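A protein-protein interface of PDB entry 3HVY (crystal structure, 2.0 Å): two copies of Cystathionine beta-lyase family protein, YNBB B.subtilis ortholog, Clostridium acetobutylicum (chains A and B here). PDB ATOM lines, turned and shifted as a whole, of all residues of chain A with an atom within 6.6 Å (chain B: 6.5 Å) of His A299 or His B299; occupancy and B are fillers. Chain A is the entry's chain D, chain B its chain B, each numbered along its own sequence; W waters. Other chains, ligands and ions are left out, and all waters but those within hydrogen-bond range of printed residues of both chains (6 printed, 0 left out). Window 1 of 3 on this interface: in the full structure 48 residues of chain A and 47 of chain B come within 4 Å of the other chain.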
ATOM      1  N   ARG A  42       0.891 -34.827  15.194  1.00  0.00           N
ATOM      2  CA  ARG A  42       0.306 -33.542  15.497  1.00  0.00           C
ATOM      3  C   ARG A  42      -0.978 -33.326  14.727  1.00  0.00           C
ATOM      4  O   ARG A  42      -1.937 -32.770  15.241  1.00  0.00           O
ATOM      5  CB  ARG A  42       1.292 -32.455  15.067  1.00  0.00           C
ATOM      6  CG  ARG A  42       0.878 -31.111  15.406  1.00  0.00           C
ATOM      7  CD  ARG A  42       1.946 -30.065  15.029  1.00  0.00           C
ATOM      8  NE  ARG A  42       2.113 -30.077  13.583  1.00  0.00           N
ATOM      9  CZ  ARG A  42       3.083 -29.473  12.909  1.00  0.00           C
ATOM     10  NH1 ARG A  42       4.010 -28.807  13.528  1.00  0.00           N
ATOM     11  NH2 ARG A  42       3.107 -29.553  11.588  1.00  0.00           N
ATOM     12  N   GLN A  46      -4.475 -32.626  16.347  1.00  0.00           N
ATOM     13  CA  GLN A  46      -5.182 -31.401  16.094  1.00  0.00           C
ATOM     14  C   GLN A  46      -6.630 -31.699  15.688  1.00  0.00           C
ATOM     15  O   GLN A  46      -7.568 -31.000  16.089  1.00  0.00           O
ATOM     16  CB  GLN A  46      -4.494 -30.573  15.006  1.00  0.00           C
ATOM     17  CG  GLN A  46      -5.238 -29.275  14.706  1.00  0.00           C
ATOM     18  CD  GLN A  46      -4.937 -28.223  15.712  1.00  0.00           C
ATOM     19  OE1 GLN A  46      -3.905 -27.568  15.626  1.00  0.00           O
ATOM     20  NE2 GLN A  46      -5.834 -28.046  16.693  1.00  0.00           N
ATOM     21  N   PHE A 224      -0.771 -35.152  24.314  1.00  0.00           N
ATOM     22  CA  PHE A 224      -0.544 -34.940  22.868  1.00  0.00           C
ATOM     23  C   PHE A 224       0.842 -35.242  22.300  1.00  0.00           C
ATOM     24  O   PHE A 224       1.101 -34.910  21.122  1.00  0.00           O
ATOM     25  CB  PHE A 224      -0.920 -33.518  22.491  1.00  0.00           C
ATOM     26  CG  PHE A 224      -2.329 -33.160  22.851  1.00  0.00           C
ATOM     27  CD1 PHE A 224      -3.377 -33.973  22.482  1.00  0.00           C
ATOM     28  CD2 PHE A 224      -2.606 -32.017  23.593  1.00  0.00           C
ATOM     29  CE1 PHE A 224      -4.691 -33.653  22.816  1.00  0.00           C
ATOM     30  CE2 PHE A 224      -3.926 -31.717  23.974  1.00  0.00           C
ATOM     31  CZ  PHE A 224      -4.953 -32.523  23.562  1.00  0.00           C
ATOM     32  N   LEU A 294      -6.308 -25.272  24.939  1.00  0.00           N
ATOM     33  CA  LEU A 294      -6.544 -26.646  24.477  1.00  0.00           C
ATOM     34  C   LEU A 294      -6.431 -26.820  22.943  1.00  0.00           C
ATOM     35  O   LEU A 294      -5.814 -27.768  22.440  1.00  0.00           O
ATOM     36  CB  LEU A 294      -7.895 -27.140  24.998  1.00  0.00           C
ATOM     37  CG  LEU A 294      -8.370 -28.532  24.610  1.00  0.00           C
ATOM     38  CD1 LEU A 294      -7.420 -29.532  25.144  1.00  0.00           C
ATOM     39  CD2 LEU A 294      -9.786 -28.825  25.059  1.00  0.00           C
ATOM     40  N   PHE A 295      -7.014 -25.895  22.202  1.00  0.00           N
ATOM     41  CA  PHE A 295      -6.949 -25.939  20.764  1.00  0.00           C
ATOM     42  C   PHE A 295      -5.533 -25.855  20.227  1.00  0.00           C
ATOM     43  O   PHE A 295      -5.188 -26.569  19.269  1.00  0.00           O
ATOM     44  CB  PHE A 295      -7.828 -24.862  20.159  1.00  0.00           C
ATOM     45  CG  PHE A 295      -8.021 -25.039  18.714  1.00  0.00           C
ATOM     46  CD1 PHE A 295      -8.813 -26.072  18.246  1.00  0.00           C
ATOM     47  CD2 PHE A 295      -7.382 -24.222  17.819  1.00  0.00           C
ATOM     48  CE1 PHE A 295      -8.987 -26.277  16.903  1.00  0.00           C
ATOM     49  CE2 PHE A 295      -7.537 -24.403  16.481  1.00  0.00           C
ATOM     50  CZ  PHE A 295      -8.342 -25.472  16.008  1.00  0.00           C
ATOM     51  N   MET A 296      -4.709 -25.013  20.851  1.00  0.00           N
ATOM     52  CA  MET A 296      -3.323 -24.849  20.444  1.00  0.00           C
ATOM     53  C   MET A 296      -2.379 -25.911  21.067  1.00  0.00           C
ATOM     54  O   MET A 296      -1.204 -25.964  20.713  1.00  0.00           O
ATOM     55  CB  MET A 296      -2.836 -23.458  20.880  1.00  0.00           C
ATOM     56  CG  MET A 296      -3.553 -22.258  20.281  1.00  0.00           C
ATOM     57  SD  MET A 296      -2.941 -20.633  21.242  1.00  0.00           S
ATOM     58  CE  MET A 296      -1.029 -21.095  21.369  1.00  0.00           C
ATOM     59  N   ALA A 297      -2.876 -26.728  21.993  1.00  0.00           N
ATOM     60  CA  ALA A 297      -2.022 -27.681  22.705  1.00  0.00           C
ATOM     61  C   ALA A 297      -1.331 -28.781  21.857  1.00  0.00           C
ATOM     62  O   ALA A 297      -0.148 -29.110  22.114  1.00  0.00           O
ATOM     63  CB  ALA A 297      -2.731 -28.268  23.896  1.00  0.00           C
ATOM     64  N   PRO A 298      -2.069 -29.411  20.927  1.00  0.00           N
ATOM     65  CA  PRO A 298      -1.404 -30.402  20.075  1.00  0.00           C
ATOM     66  C   PRO A 298      -0.223 -29.824  19.320  1.00  0.00           C
ATOM     67  O   PRO A 298       0.761 -30.499  19.093  1.00  0.00           O
ATOM     68  CB  PRO A 298      -2.513 -30.792  19.065  1.00  0.00           C
ATOM     69  CG  PRO A 298      -3.786 -30.630  19.823  1.00  0.00           C
ATOM     70  CD  PRO A 298      -3.518 -29.321  20.609  1.00  0.00           C
ATOM     71  N   HIS A 299      -0.370 -28.588  18.876  1.00  0.00           N
ATOM     72  CA  HIS A 299       0.690 -27.882  18.153  1.00  0.00           C
ATOM     73  C   HIS A 299       1.861 -27.494  19.043  1.00  0.00           C
ATOM     74  O   HIS A 299       3.016 -27.814  18.758  1.00  0.00           O
ATOM     75  CB  HIS A 299       0.121 -26.648  17.410  1.00  0.00           C
ATOM     76  CG  HIS A 299       1.121 -25.931  16.562  1.00  0.00           C
ATOM     77  ND1 HIS A 299       1.261 -26.173  15.210  1.00  0.00           N
ATOM     78  CD2 HIS A 299       2.026 -24.965  16.872  1.00  0.00           C
ATOM     79  CE1 HIS A 299       2.225 -25.398  14.735  1.00  0.00           C
ATOM     80  NE2 HIS A 299       2.703 -24.657  15.717  1.00  0.00           N
ATOM     81  N   VAL A 300       1.573 -26.760  20.081  1.00  0.00           N
ATOM     82  CA  VAL A 300       2.597 -26.312  20.995  1.00  0.00           C
ATOM     83  C   VAL A 300       3.369 -27.473  21.632  1.00  0.00           C
ATOM     84  O   VAL A 300       4.603 -27.405  21.767  1.00  0.00           O
ATOM     85  CB  VAL A 300       2.015 -25.342  22.035  1.00  0.00           C
ATOM     86  CG1 VAL A 300       3.073 -24.982  23.063  1.00  0.00           C
ATOM     87  CG2 VAL A 300       1.538 -24.029  21.298  1.00  0.00           C
ATOM     88  N   THR A 301       2.664 -28.561  21.940  1.00  0.00           N
ATOM     89  CA  THR A 301       3.308 -29.762  22.503  1.00  0.00           C
ATOM     90  C   THR A 301       4.373 -30.285  21.569  1.00  0.00           C
ATOM     91  O   THR A 301       5.488 -30.547  22.014  1.00  0.00           O
ATOM     92  CB  THR A 301       2.273 -30.861  22.848  1.00  0.00           C
ATOM     93  OG1 THR A 301       1.389 -30.380  23.866  1.00  0.00           O
ATOM     94  CG2 THR A 301       2.896 -32.200  23.246  1.00  0.00           C
ATOM     95  N   ILE A 302       4.101 -30.288  20.256  1.00  0.00           N
ATOM     96  CA  ILE A 302       5.015 -30.829  19.300  1.00  0.00           C
ATOM     97  C   ILE A 302       6.151 -29.871  19.011  1.00  0.00           C
ATOM     98  O   ILE A 302       7.242 -30.304  18.674  1.00  0.00           O
ATOM     99  CB  ILE A 302       4.279 -31.334  18.047  1.00  0.00           C
ATOM    100  CG1 ILE A 302       3.418 -32.564  18.431  1.00  0.00           C
ATOM    101  CG2 ILE A 302       5.270 -31.714  16.830  1.00  0.00           C
ATOM    102  CD1 ILE A 302       4.231 -33.815  18.838  1.00  0.00           C
ATOM    103  N   GLU A 303       5.937 -28.577  19.192  1.00  0.00           N
ATOM    104  CA  GLU A 303       7.061 -27.650  19.168  1.00  0.00           C
ATOM    105  C   GLU A 303       8.065 -28.019  20.285  1.00  0.00           C
ATOM    106  O   GLU A 303       9.282 -28.001  20.069  1.00  0.00           O
ATOM    107  CB  GLU A 303       6.604 -26.213  19.363  1.00  0.00           C
ATOM    108  CG  GLU A 303       5.729 -25.645  18.232  1.00  0.00           C
ATOM    109  CD  GLU A 303       6.439 -25.651  16.887  1.00  0.00           C
ATOM    110  OE1 GLU A 303       7.459 -24.948  16.746  1.00  0.00           O
ATOM    111  OE2 GLU A 303       5.972 -26.360  15.955  1.00  0.00           O
ATOM    112  N   ALA A 304       7.549 -28.375  21.455  1.00  0.00           N
ATOM    113  CA  ALA A 304       8.415 -28.708  22.607  1.00  0.00           C
ATOM    114  C   ALA A 304       9.097 -30.061  22.363  1.00  0.00           C
ATOM    115  O   ALA A 304      10.271 -30.215  22.642  1.00  0.00           O
ATOM    116  CB  ALA A 304       7.608 -28.693  23.885  1.00  0.00           C
ATOM    117  N   LEU A 409       7.618 -22.713  23.585  1.00  0.00           N
ATOM    118  CA  LEU A 409       6.366 -22.320  22.927  1.00  0.00           C
ATOM    119  C   LEU A 409       6.531 -22.425  21.432  1.00  0.00           C
ATOM    120  O   LEU A 409       5.555 -22.634  20.709  1.00  0.00           O
ATOM    121  CB  LEU A 409       5.958 -20.918  23.311  1.00  0.00           C
ATOM    122  CG  LEU A 409       5.644 -20.707  24.808  1.00  0.00           C
ATOM    123  CD1 LEU A 409       5.575 -19.236  25.141  1.00  0.00           C
ATOM    124  CD2 LEU A 409       4.390 -21.482  25.277  1.00  0.00           C
ATOM    125  N   THR A 410       7.763 -22.247  20.946  1.00  0.00           N
ATOM    126  CA  THR A 410       8.038 -22.451  19.536  1.00  0.00           C
ATOM    127  C   THR A 410       9.340 -23.204  19.434  1.00  0.00           C
ATOM    128  O   THR A 410      10.215 -23.162  20.356  1.00  0.00           O
ATOM    129  CB  THR A 410       8.139 -21.138  18.738  1.00  0.00           C
ATOM    130  OG1 THR A 410       9.360 -20.470  19.057  1.00  0.00           O
ATOM    131  CG2 THR A 410       6.984 -20.243  18.968  1.00  0.00           C
ATOM    132  N   PHE A 411       9.469 -23.985  18.376  1.00  0.00           N
ATOM    133  CA  PHE A 411      10.718 -24.688  18.164  1.00  0.00           C
ATOM    134  C   PHE A 411      11.875 -23.702  17.976  1.00  0.00           C
ATOM    135  O   PHE A 411      13.017 -23.948  18.427  1.00  0.00           O
ATOM    136  CB  PHE A 411      10.626 -25.611  16.933  1.00  0.00           C
ATOM    137  CG  PHE A 411      11.921 -26.184  16.528  1.00  0.00           C
ATOM    138  CD1 PHE A 411      12.602 -27.041  17.380  1.00  0.00           C
ATOM    139  CD2 PHE A 411      12.496 -25.846  15.319  1.00  0.00           C
ATOM    140  CE1 PHE A 411      13.791 -27.546  17.031  1.00  0.00           C
ATOM    141  CE2 PHE A 411      13.694 -26.342  14.967  1.00  0.00           C
ATOM    142  CZ  PHE A 411      14.358 -27.211  15.819  1.00  0.00           C
ATOM    143  N   ASP A 412      11.618 -22.615  17.276  1.00  0.00           N
ATOM    144  CA  ASP A 412      12.688 -21.629  17.086  1.00  0.00           C
ATOM    145  C   ASP A 412      13.234 -21.176  18.442  1.00  0.00           C
ATOM    146  O   ASP A 412      14.452 -21.028  18.642  1.00  0.00           O
ATOM    147  CB  ASP A 412      12.166 -20.444  16.282  1.00  0.00           C
ATOM    148  CG  ASP A 412      12.088 -20.737  14.779  1.00  0.00           C
ATOM    149  OD1 ASP A 412      13.066 -21.301  14.217  1.00  0.00           O
ATOM    150  OD2 ASP A 412      11.062 -20.409  14.134  1.00  0.00           O
ATOM    151  N   ARG B  42      11.064 -16.867   9.737  1.00  0.00           N
ATOM    152  CA  ARG B  42      10.468 -17.054  11.021  1.00  0.00           C
ATOM    153  C   ARG B  42      11.528 -17.071  12.102  1.00  0.00           C
ATOM    154  O   ARG B  42      11.382 -16.461  13.195  1.00  0.00           O
ATOM    155  CB  ARG B  42       9.646 -18.367  11.007  1.00  0.00           C
ATOM    156  CG  ARG B  42       8.980 -18.678  12.310  1.00  0.00           C
ATOM    157  CD  ARG B  42       8.263 -19.979  12.276  1.00  0.00           C
ATOM    158  NE  ARG B  42       9.213 -21.063  12.154  1.00  0.00           N
ATOM    159  CZ  ARG B  42       8.916 -22.329  11.880  1.00  0.00           C
ATOM    160  NH1 ARG B  42       7.675 -22.679  11.672  1.00  0.00           N
ATOM    161  NH2 ARG B  42       9.893 -23.247  11.791  1.00  0.00           N
ATOM    162  N   GLN B  46      11.783 -14.473  15.156  1.00  0.00           N
ATOM    163  CA  GLN B  46      11.699 -14.945  16.500  1.00  0.00           C
ATOM    164  C   GLN B  46      12.839 -14.401  17.324  1.00  0.00           C
ATOM    165  O   GLN B  46      12.661 -13.993  18.464  1.00  0.00           O
ATOM    166  CB  GLN B  46      11.760 -16.470  16.577  1.00  0.00           C
ATOM    167  CG  GLN B  46      11.625 -16.952  18.035  1.00  0.00           C
ATOM    168  CD  GLN B  46      10.207 -16.868  18.543  1.00  0.00           C
ATOM    169  OE1 GLN B  46       9.374 -17.724  18.248  1.00  0.00           O
ATOM    170  NE2 GLN B  46       9.930 -15.846  19.321  1.00  0.00           N
ATOM    171  N   PHE B 224       5.486  -9.531  10.620  1.00  0.00           N
ATOM    172  CA  PHE B 224       6.344 -10.713  10.675  1.00  0.00           C
ATOM    173  C   PHE B 224       6.245 -11.660   9.474  1.00  0.00           C
ATOM    174  O   PHE B 224       6.743 -12.773   9.535  1.00  0.00           O
ATOM    175  CB  PHE B 224       6.115 -11.503  11.978  1.00  0.00           C
ATOM    176  CG  PHE B 224       6.371 -10.709  13.221  1.00  0.00           C
ATOM    177  CD1 PHE B 224       7.605 -10.111  13.431  1.00  0.00           C
ATOM    178  CD2 PHE B 224       5.395 -10.581  14.196  1.00  0.00           C
ATOM    179  CE1 PHE B 224       7.876  -9.418  14.581  1.00  0.00           C
ATOM    180  CE2 PHE B 224       5.652  -9.858  15.350  1.00  0.00           C
ATOM    181  CZ  PHE B 224       6.911  -9.307  15.558  1.00  0.00           C
ATOM    182  N   PHE B 295       5.403 -12.529  21.579  1.00  0.00           N
ATOM    183  CA  PHE B 295       6.441 -13.550  21.509  1.00  0.00           C
ATOM    184  C   PHE B 295       6.048 -14.672  20.543  1.00  0.00           C
ATOM    185  O   PHE B 295       6.892 -15.173  19.782  1.00  0.00           O
ATOM    186  CB  PHE B 295       6.778 -14.076  22.926  1.00  0.00           C
ATOM    187  CG  PHE B 295       8.044 -14.915  22.988  1.00  0.00           C
ATOM    188  CD1 PHE B 295       9.273 -14.331  22.840  1.00  0.00           C
ATOM    189  CD2 PHE B 295       7.985 -16.286  23.172  1.00  0.00           C
ATOM    190  CE1 PHE B 295      10.422 -15.116  22.890  1.00  0.00           C
ATOM    191  CE2 PHE B 295       9.132 -17.081  23.187  1.00  0.00           C
ATOM    192  CZ  PHE B 295      10.351 -16.504  23.049  1.00  0.00           C
ATOM    193  N   MET B 296       4.776 -15.028  20.528  1.00  0.00           N
ATOM    194  CA  MET B 296       4.307 -16.128  19.693  1.00  0.00           C
ATOM    195  C   MET B 296       3.940 -15.653  18.295  1.00  0.00           C
ATOM    196  O   MET B 296       3.548 -16.460  17.466  1.00  0.00           O
ATOM    197  CB  MET B 296       3.035 -16.718  20.296  1.00  0.00           C
ATOM    198  CG  MET B 296       3.138 -17.049  21.761  1.00  0.00           C
ATOM    199  SD  MET B 296       1.568 -18.056  22.343  1.00  0.00           S
ATOM    200  CE  MET B 296       0.522 -17.057  22.776  1.00  0.00           C
ATOM    201  N   ALA B 297       3.993 -14.343  18.062  1.00  0.00           N
ATOM    202  CA  ALA B 297       3.555 -13.781  16.746  1.00  0.00           C
ATOM    203  C   ALA B 297       4.355 -14.177  15.523  1.00  0.00           C
ATOM    204  O   ALA B 297       3.778 -14.412  14.442  1.00  0.00           O
ATOM    205  CB  ALA B 297       3.447 -12.281  16.817  1.00  0.00           C
ATOM    206  N   PRO B 298       5.687 -14.142  15.620  1.00  0.00           N
ATOM    207  CA  PRO B 298       6.449 -14.592  14.464  1.00  0.00           C
ATOM    208  C   PRO B 298       6.079 -15.997  13.999  1.00  0.00           C
ATOM    209  O   PRO B 298       6.039 -16.266  12.776  1.00  0.00           O
ATOM    210  CB  PRO B 298       7.921 -14.550  14.995  1.00  0.00           C
ATOM    211  CG  PRO B 298       7.912 -13.404  15.885  1.00  0.00           C
ATOM    212  CD  PRO B 298       6.593 -13.639  16.666  1.00  0.00           C
ATOM    213  N   HIS B 299       5.865 -16.891  14.965  1.00  0.00           N
ATOM    214  CA  HIS B 299       5.485 -18.264  14.685  1.00  0.00           C
ATOM    215  C   HIS B 299       4.084 -18.401  14.118  1.00  0.00           C
ATOM    216  O   HIS B 299       3.882 -18.987  13.059  1.00  0.00           O
ATOM    217  CB  HIS B 299       5.641 -19.106  15.964  1.00  0.00           C
ATOM    218  CG  HIS B 299       5.344 -20.555  15.745  1.00  0.00           C
ATOM    219  ND1 HIS B 299       6.313 -21.469  15.390  1.00  0.00           N
ATOM    220  CD2 HIS B 299       4.175 -21.233  15.785  1.00  0.00           C
ATOM    221  CE1 HIS B 299       5.741 -22.654  15.224  1.00  0.00           C
ATOM    222  NE2 HIS B 299       4.454 -22.542  15.473  1.00  0.00           N
ATOM    223  N   VAL B 300       3.105 -17.837  14.808  1.00  0.00           N
ATOM    224  CA  VAL B 300       1.713 -17.972  14.410  1.00  0.00           C
ATOM    225  C   VAL B 300       1.490 -17.354  13.042  1.00  0.00           C
ATOM    226  O   VAL B 300       0.794 -17.913  12.222  1.00  0.00           O
ATOM    227  CB  VAL B 300       0.733 -17.405  15.477  1.00  0.00           C
ATOM    228  CG1 VAL B 300      -0.727 -17.458  14.992  1.00  0.00           C
ATOM    229  CG2 VAL B 300       0.854 -18.247  16.824  1.00  0.00           C
ATOM    230  N   THR B 301       2.138 -16.229  12.793  1.00  0.00           N
ATOM    231  CA  THR B 301       2.055 -15.535  11.512  1.00  0.00           C
ATOM    232  C   THR B 301       2.485 -16.474  10.386  1.00  0.00           C
ATOM    233  O   THR B 301       1.833 -16.566   9.310  1.00  0.00           O
ATOM    234  CB  THR B 301       2.942 -14.277  11.499  1.00  0.00           C
ATOM    235  OG1 THR B 301       2.429 -13.335  12.428  1.00  0.00           O
ATOM    236  CG2 THR B 301       2.981 -13.650  10.106  1.00  0.00           C
ATOM    237  N   ILE B 302       3.584 -17.184  10.593  1.00  0.00           N
ATOM    238  CA  ILE B 302       4.103 -18.086   9.560  1.00  0.00           C
ATOM    239  C   ILE B 302       3.231 -19.354   9.382  1.00  0.00           C
ATOM    240  O   ILE B 302       3.132 -19.886   8.272  1.00  0.00           O
ATOM    241  CB  ILE B 302       5.662 -18.324   9.766  1.00  0.00           C
ATOM    242  CG1 ILE B 302       6.417 -17.003   9.493  1.00  0.00           C
ATOM    243  CG2 ILE B 302       6.215 -19.450   8.865  1.00  0.00           C
ATOM    244  CD1 ILE B 302       6.371 -16.501   7.985  1.00  0.00           C
ATOM    245  N   GLU B 303       2.561 -19.789  10.447  1.00  0.00           N
ATOM    246  CA  GLU B 303       1.557 -20.830  10.315  1.00  0.00           C
ATOM    247  C   GLU B 303       0.479 -20.361   9.332  1.00  0.00           C
ATOM    248  O   GLU B 303       0.041 -21.148   8.434  1.00  0.00           O
ATOM    249  CB  GLU B 303       0.928 -21.152  11.661  1.00  0.00           C
ATOM    250  CG  GLU B 303       1.885 -21.782  12.690  1.00  0.00           C
ATOM    251  CD  GLU B 303       2.469 -23.111  12.224  1.00  0.00           C
ATOM    252  OE1 GLU B 303       1.678 -24.072  12.031  1.00  0.00           O
ATOM    253  OE2 GLU B 303       3.710 -23.221  12.057  1.00  0.00           O
ATOM    254  N   ALA B 304       0.052 -19.103   9.489  1.00  0.00           N
ATOM    255  CA  ALA B 304      -1.008 -18.550   8.632  1.00  0.00           C
ATOM    256  C   ALA B 304      -0.476 -18.406   7.234  1.00  0.00           C
ATOM    257  O   ALA B 304      -1.192 -18.679   6.303  1.00  0.00           O
ATOM    258  CB  ALA B 304      -1.588 -17.197   9.142  1.00  0.00           C
ATOM    259  N   LEU B 409      -4.432 -20.511  13.317  1.00  0.00           N
ATOM    260  CA  LEU B 409      -3.595 -20.510  14.515  1.00  0.00           C
ATOM    261  C   LEU B 409      -2.473 -21.569  14.370  1.00  0.00           C
ATOM    262  O   LEU B 409      -1.366 -21.414  14.928  1.00  0.00           O
ATOM    263  CB  LEU B 409      -4.458 -20.763  15.726  1.00  0.00           C
ATOM    264  CG  LEU B 409      -5.380 -19.635  16.218  1.00  0.00           C
ATOM    265  CD1 LEU B 409      -6.109 -20.087  17.451  1.00  0.00           C
ATOM    266  CD2 LEU B 409      -4.525 -18.378  16.504  1.00  0.00           C
ATOM    267  N   THR B 410      -2.774 -22.661  13.654  1.00  0.00           N
ATOM    268  CA  THR B 410      -1.769 -23.678  13.319  1.00  0.00           C
ATOM    269  C   THR B 410      -1.961 -24.010  11.834  1.00  0.00           C
ATOM    270  O   THR B 410      -3.035 -23.831  11.314  1.00  0.00           O
ATOM    271  CB  THR B 410      -1.939 -24.898  14.174  1.00  0.00           C
ATOM    272  OG1 THR B 410      -3.115 -25.622  13.750  1.00  0.00           O
ATOM    273  CG2 THR B 410      -1.976 -24.494  15.705  1.00  0.00           C
ATOM    274  N   PHE B 411      -0.913 -24.459  11.148  1.00  0.00           N
ATOM    275  CA  PHE B 411      -1.034 -24.862   9.762  1.00  0.00           C
ATOM    276  C   PHE B 411      -1.959 -26.062   9.650  1.00  0.00           C
ATOM    277  O   PHE B 411      -2.743 -26.172   8.706  1.00  0.00           O
ATOM    278  CB  PHE B 411       0.372 -25.169   9.151  1.00  0.00           C
ATOM    279  CG  PHE B 411       0.321 -25.852   7.826  1.00  0.00           C
ATOM    280  CD1 PHE B 411      -0.181 -25.206   6.705  1.00  0.00           C
ATOM    281  CD2 PHE B 411       0.783 -27.145   7.687  1.00  0.00           C
ATOM    282  CE1 PHE B 411      -0.244 -25.853   5.489  1.00  0.00           C
ATOM    283  CE2 PHE B 411       0.737 -27.784   6.482  1.00  0.00           C
ATOM    284  CZ  PHE B 411       0.218 -27.146   5.374  1.00  0.00           C
ATOM    285  N   ASP B 412      -1.901 -26.968  10.621  1.00  0.00           N
ATOM    286  CA  ASP B 412      -2.813 -28.125  10.594  1.00  0.00           C
ATOM    287  C   ASP B 412      -4.279 -27.712  10.500  1.00  0.00           C
ATOM    288  O   ASP B 412      -5.059 -28.293   9.737  1.00  0.00           O
ATOM    289  CB  ASP B 412      -2.575 -28.998  11.826  1.00  0.00           C
ATOM    290  CG  ASP B 412      -1.328 -29.845  11.721  1.00  0.00           C
ATOM    291  OD1 ASP B 412      -1.073 -30.425  10.638  1.00  0.00           O
ATOM    292  OD2 ASP B 412      -0.610 -29.993  12.746  1.00  0.00           O
HETATM  293  O   HOH W   1       9.100 -22.205  15.384  1.00  0.00           O
HETATM  294  O   HOH W   2       1.355 -31.745  10.665  1.00  0.00           O
HETATM  295  O   HOH W   3       9.046 -19.240  15.740  1.00  0.00           O
HETATM  296  O   HOH W   4       0.530 -27.210  12.491  1.00  0.00           O
HETATM  297  O   HOH W   5      12.551 -21.789  11.743  1.00  0.00           O
HETATM  298  O   HOH W   6      -1.213 -28.327  14.810  1.00  0.00           O
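The guanidinium group (NE) of Arg B42 lies within salt-bridge range of the side-chain carboxylate (OD2) of Asp A412, 2.8 Å away. OG1 of Thr A410 is in hydrogen-bond range of OE1 of Gln B46. A ring nitrogen (NE2) of His B299 is in hydrogen-bond range of a ring nitrogen (NE2) of His A299. The side-chain hydroxyl (OG1) of Thr B410 lies within hydrogen-bond range of the side-chain amide oxygen (OE1) of Gln A46, at 2.8 Å. The guanidinium group (NE) of Arg A42 is in salt-bridge range of the side-chain carboxylate (OD2) of Asp B412 (2.8 Å).
The side-chain amide nitrogen (NE2) of Gln B46 lies within hydrogen-bond range of the backbone carbonyl oxygen (O) of Phe B295, 3.1 Å away. OE1 of Glu B303 is in hydrogen-bond range of N of Phe B411 (2.8 Å). The side-chain carboxylate (OE2) of Glu A303 lies within salt-bridge range of the guanidinium group (NH1) of Arg A42 (3.97 Å). The side-chain amide nitrogen of Gln A46 is in hydrogen-bond range of the backbone carbonyl oxygen of Phe A295. The side-chain carboxylate of Glu A303 lies within hydrogen-bond range of the backbone NH of Phe A411 (2.8 Å).
Among the printed residues, merely in contact across the chains: Gln A46 with Asp B412, His A299 with Glu B303, His A299 with Thr B410, Glu A303 with His B299, Thr A410 with His B299 and Asp A412 with Gln B46.
Printed residues of chain B within 4 Å of His A299: His B299, Glu B303 and Thr B410. His B299 touches just these residues of chain A: His A299 (2.8 Å), Glu A303 (3.2 Å) and Thr A410 (3.5 Å). Printed residues of chain B within 4 Å of Arg A42: Asp B412. Of the printed residues of chain A, Asp B412 touches Arg A42 (2.8 Å) and Gln A46 (3.9 Å). Thr B301 touches none of the printed residues of chain A. Ala B297 touches none of the printed residues of chain A. The nearest residue of chain B that does not touch His A299 is Phe B411 (4.9 Å). The nearest printed residue of chain A that does not touch Arg B42 is Phe A411 (5.1 Å).
Of the 18 printed residues of chain A, 6 touch a printed residue of chain B. Printed residues of chain A that touch a printed residue of chain B: Arg A42, Gln A46, His A299, Glu A303, Thr A410 and Asp A412. Hydrophobic or aromatic side chains of chain A that line the printed part of chain B: His A299. Of the 17 printed residues of chain B, 6 touch a printed residue of chain A. Among the printed residues, 11 pairs touch across the chains.
Arg A42 touches Asp B412, and with the chains exchanged Asp A412 touches Arg B42. Gln A46 touches Thr B410, and with the chains exchanged Thr A410 touches Gln B46. His A299 touches its own counterpart, His B299. His A299 touches Glu B303, and with the chains exchanged Glu A303 touches His B299. 17 positions are printed for both chains.
Water W5 bridges the side-chain carboxylate of Asp A412 (2.6 Å) and the guanidinium group of Arg B42 (3.0 Å). Water W6 lies within hydrogen-bond range of OD2 of Asp B412 (2.7 Å), OE1 of Gln A46 (2.9 Å), ND1 of His A299 (3.3 Å) and OG1 of Thr B410 (3.5 Å). Water W2 lies within hydrogen-bond range of the side-chain carboxylate (OD1) of Asp B412 (2.8 Å) and the guanidinium group (NH2) of Arg A42 (3.0 Å). Water W3 bridges OD2 of Asp A412 (2.8 Å) and OE1 of Gln B46 (2.9 Å). Water W1 lies within hydrogen-bond range of ND1 of His B299 (2.9 Å), OD2 of Asp A412 (2.9 Å), NE of Arg B42 (3.4 Å) and OE1 of Glu A303 (3.5 Å). Water W4 lies within hydrogen-bond range of a ring nitrogen (ND1) of His A299 (3.0 Å), the side-chain carboxylate of Asp B412 (3.0 Å), the side-chain carboxylate of Glu B303 (3.4 Å), the backbone NH of Phe B411 (3.4 Å) and the guanidinium group of Arg A42 (3.5 Å).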
